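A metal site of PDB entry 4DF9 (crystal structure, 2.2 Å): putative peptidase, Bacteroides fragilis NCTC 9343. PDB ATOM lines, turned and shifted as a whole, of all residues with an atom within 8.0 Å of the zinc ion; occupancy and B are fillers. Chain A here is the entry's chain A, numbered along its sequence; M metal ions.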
ATOM      1  N   LEU A 303      -3.717  18.266  -0.941  1.00  0.00           N
ATOM      2  CA  LEU A 303      -3.632  16.811  -0.992  1.00  0.00           C
ATOM      3  C   LEU A 303      -4.115  16.185   0.313  1.00  0.00           C
ATOM      4  O   LEU A 303      -3.973  16.772   1.384  1.00  0.00           O
ATOM      5  CB  LEU A 303      -2.201  16.345  -1.304  1.00  0.00           C
ATOM      6  CG  LEU A 303      -1.615  16.794  -2.642  1.00  0.00           C
ATOM      7  CD1 LEU A 303      -0.100  16.576  -2.661  1.00  0.00           C
ATOM      8  CD2 LEU A 303      -2.323  16.125  -3.819  1.00  0.00           C
ATOM      9  N   ALA A 304      -4.692  14.993   0.207  1.00  0.00           N
ATOM     10  CA  ALA A 304      -5.147  14.224   1.379  1.00  0.00           C
ATOM     11  C   ALA A 304      -4.008  13.361   1.887  1.00  0.00           C
ATOM     12  O   ALA A 304      -3.050  13.106   1.160  1.00  0.00           O
ATOM     13  CB  ALA A 304      -6.318  13.330   0.996  1.00  0.00           C
ATOM     14  N   ASP A 305      -4.145  12.881   3.122  1.00  0.00           N
ATOM     15  CA  ASP A 305      -3.192  11.922   3.669  1.00  0.00           C
ATOM     16  C   ASP A 305      -3.471  10.587   3.023  1.00  0.00           C
ATOM     17  O   ASP A 305      -4.645  10.235   2.808  1.00  0.00           O
ATOM     18  CB  ASP A 305      -3.342  11.838   5.194  1.00  0.00           C
ATOM     19  CG  ASP A 305      -2.690  13.000   5.892  1.00  0.00           C
ATOM     20  OD1 ASP A 305      -1.520  13.317   5.564  1.00  0.00           O
ATOM     21  OD2 ASP A 305      -3.344  13.612   6.763  1.00  0.00           O
ATOM     22  N   GLU A 306      -2.410   9.848   2.649  1.00  0.00           N
ATOM     23  CA  GLU A 306      -2.550   8.551   2.009  1.00  0.00           C
ATOM     24  C   GLU A 306      -2.320   7.418   3.010  1.00  0.00           C
ATOM     25  O   GLU A 306      -2.479   6.240   2.660  1.00  0.00           O
ATOM     26  CB  GLU A 306      -1.595   8.441   0.811  1.00  0.00           C
ATOM     27  CG  GLU A 306      -1.999   9.310  -0.369  1.00  0.00           C
ATOM     28  CD  GLU A 306      -1.019   9.209  -1.525  1.00  0.00           C
ATOM     29  OE1 GLU A 306      -0.359   8.155  -1.660  1.00  0.00           O
ATOM     30  OE2 GLU A 306      -0.941  10.163  -2.318  1.00  0.00           O
ATOM     31  N   GLN A 327      -7.484  15.153  -4.718  1.00  0.00           N
ATOM     32  CA  GLN A 327      -7.078  14.540  -5.979  1.00  0.00           C
ATOM     33  C   GLN A 327      -6.270  13.248  -5.893  1.00  0.00           C
ATOM     34  O   GLN A 327      -6.151  12.561  -6.911  1.00  0.00           O
ATOM     35  CB  GLN A 327      -6.277  15.588  -6.769  1.00  0.00           C
ATOM     36  CG  GLN A 327      -7.074  16.870  -7.013  1.00  0.00           C
ATOM     37  CD  GLN A 327      -8.216  16.649  -7.970  1.00  0.00           C
ATOM     38  OE1 GLN A 327      -8.019  16.499  -9.169  1.00  0.00           O
ATOM     39  NE2 GLN A 327      -9.425  16.577  -7.472  1.00  0.00           N
ATOM     40  N   ASN A 328      -5.718  12.923  -4.719  1.00  0.00           N
ATOM     41  CA  ASN A 328      -4.855  11.749  -4.574  1.00  0.00           C
ATOM     42  C   ASN A 328      -5.521  10.620  -3.761  1.00  0.00           C
ATOM     43  O   ASN A 328      -4.832   9.692  -3.355  1.00  0.00           O
ATOM     44  CB  ASN A 328      -3.535  12.167  -3.917  1.00  0.00           C
ATOM     45  CG  ASN A 328      -3.702  12.763  -2.524  1.00  0.00           C
ATOM     46  OD1 ASN A 328      -4.629  13.530  -2.261  1.00  0.00           O
ATOM     47  ND2 ASN A 328      -2.812  12.434  -1.622  1.00  0.00           N
ATOM     48  N   ILE A 329      -6.845  10.707  -3.520  1.00  0.00           N
ATOM     49  CA  ILE A 329      -7.589   9.611  -2.885  1.00  0.00           C
ATOM     50  C   ILE A 329      -8.887   9.434  -3.645  1.00  0.00           C
ATOM     51  O   ILE A 329      -9.389  10.394  -4.246  1.00  0.00           O
ATOM     52  CB  ILE A 329      -7.825   9.759  -1.341  1.00  0.00           C
ATOM     53  CG1 ILE A 329      -8.567  11.066  -0.983  1.00  0.00           C
ATOM     54  CG2 ILE A 329      -6.523   9.502  -0.507  1.00  0.00           C
ATOM     55  CD1 ILE A 329      -9.200  11.087   0.448  1.00  0.00           C
ATOM     56  N   ARG A 376      -5.567   4.888  -2.711  1.00  0.00           N
ATOM     57  CA  ARG A 376      -4.488   5.828  -2.988  1.00  0.00           C
ATOM     58  C   ARG A 376      -3.821   5.453  -4.351  1.00  0.00           C
ATOM     59  O   ARG A 376      -4.031   4.346  -4.858  1.00  0.00           O
ATOM     60  CB  ARG A 376      -3.492   5.880  -1.809  1.00  0.00           C
ATOM     61  CG  ARG A 376      -2.697   4.594  -1.635  1.00  0.00           C
ATOM     62  CD  ARG A 376      -1.951   4.556  -0.313  1.00  0.00           C
ATOM     63  NE  ARG A 376      -1.048   3.407  -0.295  1.00  0.00           N
ATOM     64  CZ  ARG A 376      -1.414   2.168   0.025  1.00  0.00           C
ATOM     65  NH1 ARG A 376      -2.677   1.922   0.370  1.00  0.00           N
ATOM     66  NH2 ARG A 376      -0.534   1.182   0.010  1.00  0.00           N
ATOM     67  N   PRO A 377      -3.052   6.382  -4.990  1.00  0.00           N
ATOM     68  CA  PRO A 377      -2.560   6.125  -6.346  1.00  0.00           C
ATOM     69  C   PRO A 377      -1.296   5.267  -6.485  1.00  0.00           C
ATOM     70  O   PRO A 377      -0.978   4.838  -7.599  1.00  0.00           O
ATOM     71  CB  PRO A 377      -2.284   7.532  -6.882  1.00  0.00           C
ATOM     72  CG  PRO A 377      -2.908   8.488  -5.874  1.00  0.00           C
ATOM     73  CD  PRO A 377      -2.759   7.766  -4.590  1.00  0.00           C
ATOM     74  N   ALA A 378      -0.541   5.076  -5.396  1.00  0.00           N
ATOM     75  CA  ALA A 378       0.695   4.289  -5.436  1.00  0.00           C
ATOM     76  C   ALA A 378       0.840   3.571  -4.114  1.00  0.00           C
ATOM     77  O   ALA A 378       0.177   3.984  -3.147  1.00  0.00           O
ATOM     78  CB  ALA A 378       1.891   5.200  -5.671  1.00  0.00           C
ATOM     79  N   ASP A 380       3.354   3.561  -2.046  1.00  0.00           N
ATOM     80  CA  ASP A 380       3.944   4.503  -1.108  1.00  0.00           C
ATOM     81  C   ASP A 380       4.087   5.889  -1.770  1.00  0.00           C
ATOM     82  O   ASP A 380       4.050   6.008  -3.011  1.00  0.00           O
ATOM     83  CB  ASP A 380       5.280   3.970  -0.571  1.00  0.00           C
ATOM     84  CG  ASP A 380       5.611   4.402   0.850  1.00  0.00           C
ATOM     85  OD1 ASP A 380       5.026   5.413   1.331  1.00  0.00           O
ATOM     86  OD2 ASP A 380       6.468   3.762   1.494  1.00  0.00           O
ATOM     87  N   CYS A 381       4.223   6.933  -0.935  1.00  0.00           N
ATOM     88  CA  CYS A 381       4.242   8.348  -1.326  1.00  0.00           C
ATOM     89  C   CYS A 381       4.681   9.176  -0.149  1.00  0.00           C
ATOM     90  O   CYS A 381       4.492   8.775   0.991  1.00  0.00           O
ATOM     91  CB  CYS A 381       2.840   8.744  -1.789  1.00  0.00           C
ATOM     92  SG  CYS A 381       2.643  10.479  -2.273  1.00  0.00           S
ATOM     93  N   ARG A 382       5.138  10.414  -0.431  1.00  0.00           N
ATOM     94  CA  ARG A 382       5.432  11.422   0.600  1.00  0.00           C
ATOM     95  C   ARG A 382       4.160  11.693   1.425  1.00  0.00           C
ATOM     96  O   ARG A 382       4.251  12.041   2.610  1.00  0.00           O
ATOM     97  CB  ARG A 382       5.919  12.728  -0.073  1.00  0.00           C
ATOM     98  CG  ARG A 382       5.837  14.042   0.773  1.00  0.00           C
ATOM     99  CD  ARG A 382       6.919  14.203   1.848  1.00  0.00           C
ATOM    100  NE  ARG A 382       8.267  13.971   1.326  1.00  0.00           N
ATOM    101  CZ  ARG A 382       8.976  12.862   1.540  1.00  0.00           C
ATOM    102  NH1 ARG A 382       8.494  11.899   2.323  1.00  0.00           N
ATOM    103  NH2 ARG A 382      10.169  12.721   0.995  1.00  0.00           N
ATOM    104  N   MET A 383       2.971  11.522   0.804  1.00  0.00           N
ATOM    105  CA  MET A 383       1.695  11.765   1.526  1.00  0.00           C
ATOM    106  C   MET A 383       1.282  10.577   2.390  1.00  0.00           C
ATOM    107  O   MET A 383       0.300  10.679   3.123  1.00  0.00           O
ATOM    108  CB  MET A 383       0.569  12.164   0.549  1.00  0.00           C
ATOM    109  CG  MET A 383       0.809  13.550  -0.133  1.00  0.00           C
ATOM    110  SD  MET A 383       1.391  14.962   1.069  1.00  0.00           S
ATOM    111  CE  MET A 383      -0.146  15.191   2.110  1.00  0.00           C
ATOM    112  N   ARG A 384       2.033   9.468   2.314  1.00  0.00           N
ATOM    113  CA  ARG A 384       1.786   8.292   3.141  1.00  0.00           C
ATOM    114  C   ARG A 384       2.864   8.105   4.253  1.00  0.00           C
ATOM    115  O   ARG A 384       2.518   7.836   5.401  1.00  0.00           O
ATOM    116  CB  ARG A 384       1.720   7.054   2.274  1.00  0.00           C
ATOM    117  CG  ARG A 384       1.214   5.872   3.045  1.00  0.00           C
ATOM    118  CD  ARG A 384       1.364   4.599   2.299  1.00  0.00           C
ATOM    119  NE  ARG A 384       1.004   3.497   3.173  1.00  0.00           N
ATOM    120  CZ  ARG A 384       1.494   2.265   3.081  1.00  0.00           C
ATOM    121  NH1 ARG A 384       2.340   1.952   2.112  1.00  0.00           N
ATOM    122  NH2 ARG A 384       1.097   1.328   3.939  1.00  0.00           N
ATOM    123  N   TYR A 388       9.586   7.512   2.539  1.00  0.00           N
ATOM    124  CA  TYR A 388       9.510   7.455   1.082  1.00  0.00           C
ATOM    125  C   TYR A 388      10.054   8.764   0.494  1.00  0.00           C
ATOM    126  O   TYR A 388       9.746   9.831   1.026  1.00  0.00           O
ATOM    127  CB  TYR A 388       8.076   7.165   0.613  1.00  0.00           C
ATOM    128  CG  TYR A 388       8.039   6.664  -0.809  1.00  0.00           C
ATOM    129  CD1 TYR A 388       8.402   5.348  -1.105  1.00  0.00           C
ATOM    130  CD2 TYR A 388       7.723   7.509  -1.867  1.00  0.00           C
ATOM    131  CE1 TYR A 388       8.408   4.877  -2.423  1.00  0.00           C
ATOM    132  CE2 TYR A 388       7.722   7.055  -3.187  1.00  0.00           C
ATOM    133  CZ  TYR A 388       8.065   5.741  -3.453  1.00  0.00           C
ATOM    134  OH  TYR A 388       8.056   5.281  -4.739  1.00  0.00           O
ATOM    135  N   THR A 390       9.723  10.508  -2.499  1.00  0.00           N
ATOM    136  CA  THR A 390       9.046  11.423  -3.431  1.00  0.00           C
ATOM    137  C   THR A 390       7.525  11.410  -3.332  1.00  0.00           C
ATOM    138  O   THR A 390       6.956  10.481  -2.792  1.00  0.00           O
ATOM    139  CB  THR A 390       9.372  10.995  -4.903  1.00  0.00           C
ATOM    140  OG1 THR A 390       8.877   9.671  -5.118  1.00  0.00           O
ATOM    141  CG2 THR A 390      10.872  11.050  -5.240  1.00  0.00           C
ATOM    142  N   PHE A 391       6.887  12.411  -3.974  1.00  0.00           N
ATOM    143  CA  PHE A 391       5.430  12.415  -4.186  1.00  0.00           C
ATOM    144  C   PHE A 391       5.164  11.385  -5.236  1.00  0.00           C
ATOM    145  O   PHE A 391       5.949  11.275  -6.184  1.00  0.00           O
ATOM    146  CB  PHE A 391       4.928  13.792  -4.677  1.00  0.00           C
ATOM    147  CG  PHE A 391       4.857  14.862  -3.614  1.00  0.00           C
ATOM    148  CD1 PHE A 391       3.798  14.891  -2.717  1.00  0.00           C
ATOM    149  CD2 PHE A 391       5.817  15.850  -3.531  1.00  0.00           C
ATOM    150  CE1 PHE A 391       3.718  15.896  -1.738  1.00  0.00           C
ATOM    151  CE2 PHE A 391       5.727  16.875  -2.562  1.00  0.00           C
ATOM    152  CZ  PHE A 391       4.681  16.872  -1.662  1.00  0.00           C
ATOM    153  N   CYS A 392       4.060  10.645  -5.124  1.00  0.00           N
ATOM    154  CA  CYS A 392       3.677   9.671  -6.144  1.00  0.00           C
ATOM    155  C   CYS A 392       3.351  10.421  -7.473  1.00  0.00           C
ATOM    156  O   CYS A 392       3.159  11.655  -7.431  1.00  0.00           O
ATOM    157  CB  CYS A 392       2.515   8.805  -5.670  1.00  0.00           C
ATOM    158  SG  CYS A 392       0.907   9.650  -5.608  1.00  0.00           S
ATOM    159  N   PRO A 393       3.310   9.749  -8.650  1.00  0.00           N
ATOM    160  CA  PRO A 393       3.040  10.481  -9.902  1.00  0.00           C
ATOM    161  C   PRO A 393       1.713  11.242  -9.925  1.00  0.00           C
ATOM    162  O   PRO A 393       1.625  12.247 -10.617  1.00  0.00           O
ATOM    163  CB  PRO A 393       3.051   9.369 -10.953  1.00  0.00           C
ATOM    164  CG  PRO A 393       3.952   8.336 -10.377  1.00  0.00           C
ATOM    165  CD  PRO A 393       3.594   8.328  -8.923  1.00  0.00           C
ATOM    166  N   VAL A 394       0.709  10.777  -9.180  1.00  0.00           N
ATOM    167  CA  VAL A 394      -0.582  11.446  -9.153  1.00  0.00           C
ATOM    168  C   VAL A 394      -0.515  12.734  -8.299  1.00  0.00           C
ATOM    169  O   VAL A 394      -1.064  13.750  -8.710  1.00  0.00           O
ATOM    170  CB  VAL A 394      -1.681  10.482  -8.709  1.00  0.00           C
ATOM    171  CG1 VAL A 394      -3.012  11.194  -8.421  1.00  0.00           C
ATOM    172  CG2 VAL A 394      -1.856   9.393  -9.770  1.00  0.00           C
ATOM    173  N   CYS A 395       0.208  12.700  -7.162  1.00  0.00           N
ATOM    174  CA  CYS A 395       0.404  13.888  -6.327  1.00  0.00           C
ATOM    175  C   CYS A 395       1.197  14.931  -7.128  1.00  0.00           C
ATOM    176  O   CYS A 395       0.861  16.118  -7.095  1.00  0.00           O
ATOM    177  CB  CYS A 395       1.109  13.535  -5.020  1.00  0.00           C
ATOM    178  SG  CYS A 395       0.031  12.759  -3.774  1.00  0.00           S
ATOM    179  N   GLN A 396       2.206  14.472  -7.896  1.00  0.00           N
ATOM    180  CA  GLN A 396       3.031  15.342  -8.729  1.00  0.00           C
ATOM    181  C   GLN A 396       2.166  16.057  -9.795  1.00  0.00           C
ATOM    182  O   GLN A 396       2.310  17.257  -9.958  1.00  0.00           O
ATOM    183  CB  GLN A 396       4.144  14.537  -9.391  1.00  0.00           C
ATOM    184  CG  GLN A 396       5.254  14.182  -8.412  1.00  0.00           C
ATOM    185  CD  GLN A 396       6.469  13.635  -9.104  1.00  0.00           C
ATOM    186  OE1 GLN A 396       6.816  14.072 -10.221  1.00  0.00           O
ATOM    187  NE2 GLN A 396       7.162  12.716  -8.442  1.00  0.00           N
ATOM    188  N   ALA A 398      -1.120  16.586  -9.585  1.00  0.00           N
ATOM    189  CA  ALA A 398      -2.029  17.438  -8.819  1.00  0.00           C
ATOM    190  C   ALA A 398      -1.335  18.754  -8.419  1.00  0.00           C
ATOM    191  O   ALA A 398      -1.915  19.818  -8.603  1.00  0.00           O
ATOM    192  CB  ALA A 398      -2.541  16.696  -7.593  1.00  0.00           C
ATOM    193  N   ILE A 399      -0.083  18.678  -7.921  1.00  0.00           N
ATOM    194  CA  ILE A 399       0.699  19.857  -7.544  1.00  0.00           C
ATOM    195  C   ILE A 399       0.998  20.722  -8.794  1.00  0.00           C
ATOM    196  O   ILE A 399       0.836  21.946  -8.731  1.00  0.00           O
ATOM    197  CB  ILE A 399       1.998  19.490  -6.770  1.00  0.00           C
ATOM    198  CG1 ILE A 399       1.655  18.805  -5.400  1.00  0.00           C
ATOM    199  CG2 ILE A 399       2.894  20.734  -6.549  1.00  0.00           C
ATOM    200  CD1 ILE A 399       2.802  17.921  -4.836  1.00  0.00           C
HETATM  201 ZN    ZN M   1       0.664  10.617  -3.539  1.00  0.00          ZN
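The side-chain carboxylate of Glu 306 lies close to the side-chain amide nitrogen of Asn 328, 3.0 Å away. The backbone carbonyl oxygen of Met 383 lies within hydrogen-bond range of the backbone NH of Glu 306 (2.9 Å). The side-chain sulfur (SG) of Cys 381 sits close to the backbone NH (N) of Met 383, at 3.3 Å. The side-chain sulfur of Cys 395 lies close to the side-chain amide nitrogen of Asn 328, at 3.6 Å. SG of Cys 392 sits close to N of Val 394 (3.8 Å).
The zinc ion is bound by the side-chain carboxylate (OE2) of Glu 306 (2.1 Å), the side-chain sulfur (SG) of Cys 395 (2.2 Å), the side-chain sulfur (SG) of Cys 392 (2.3 Å) and the side-chain sulfur (SG) of Cys 381 (2.4 Å).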
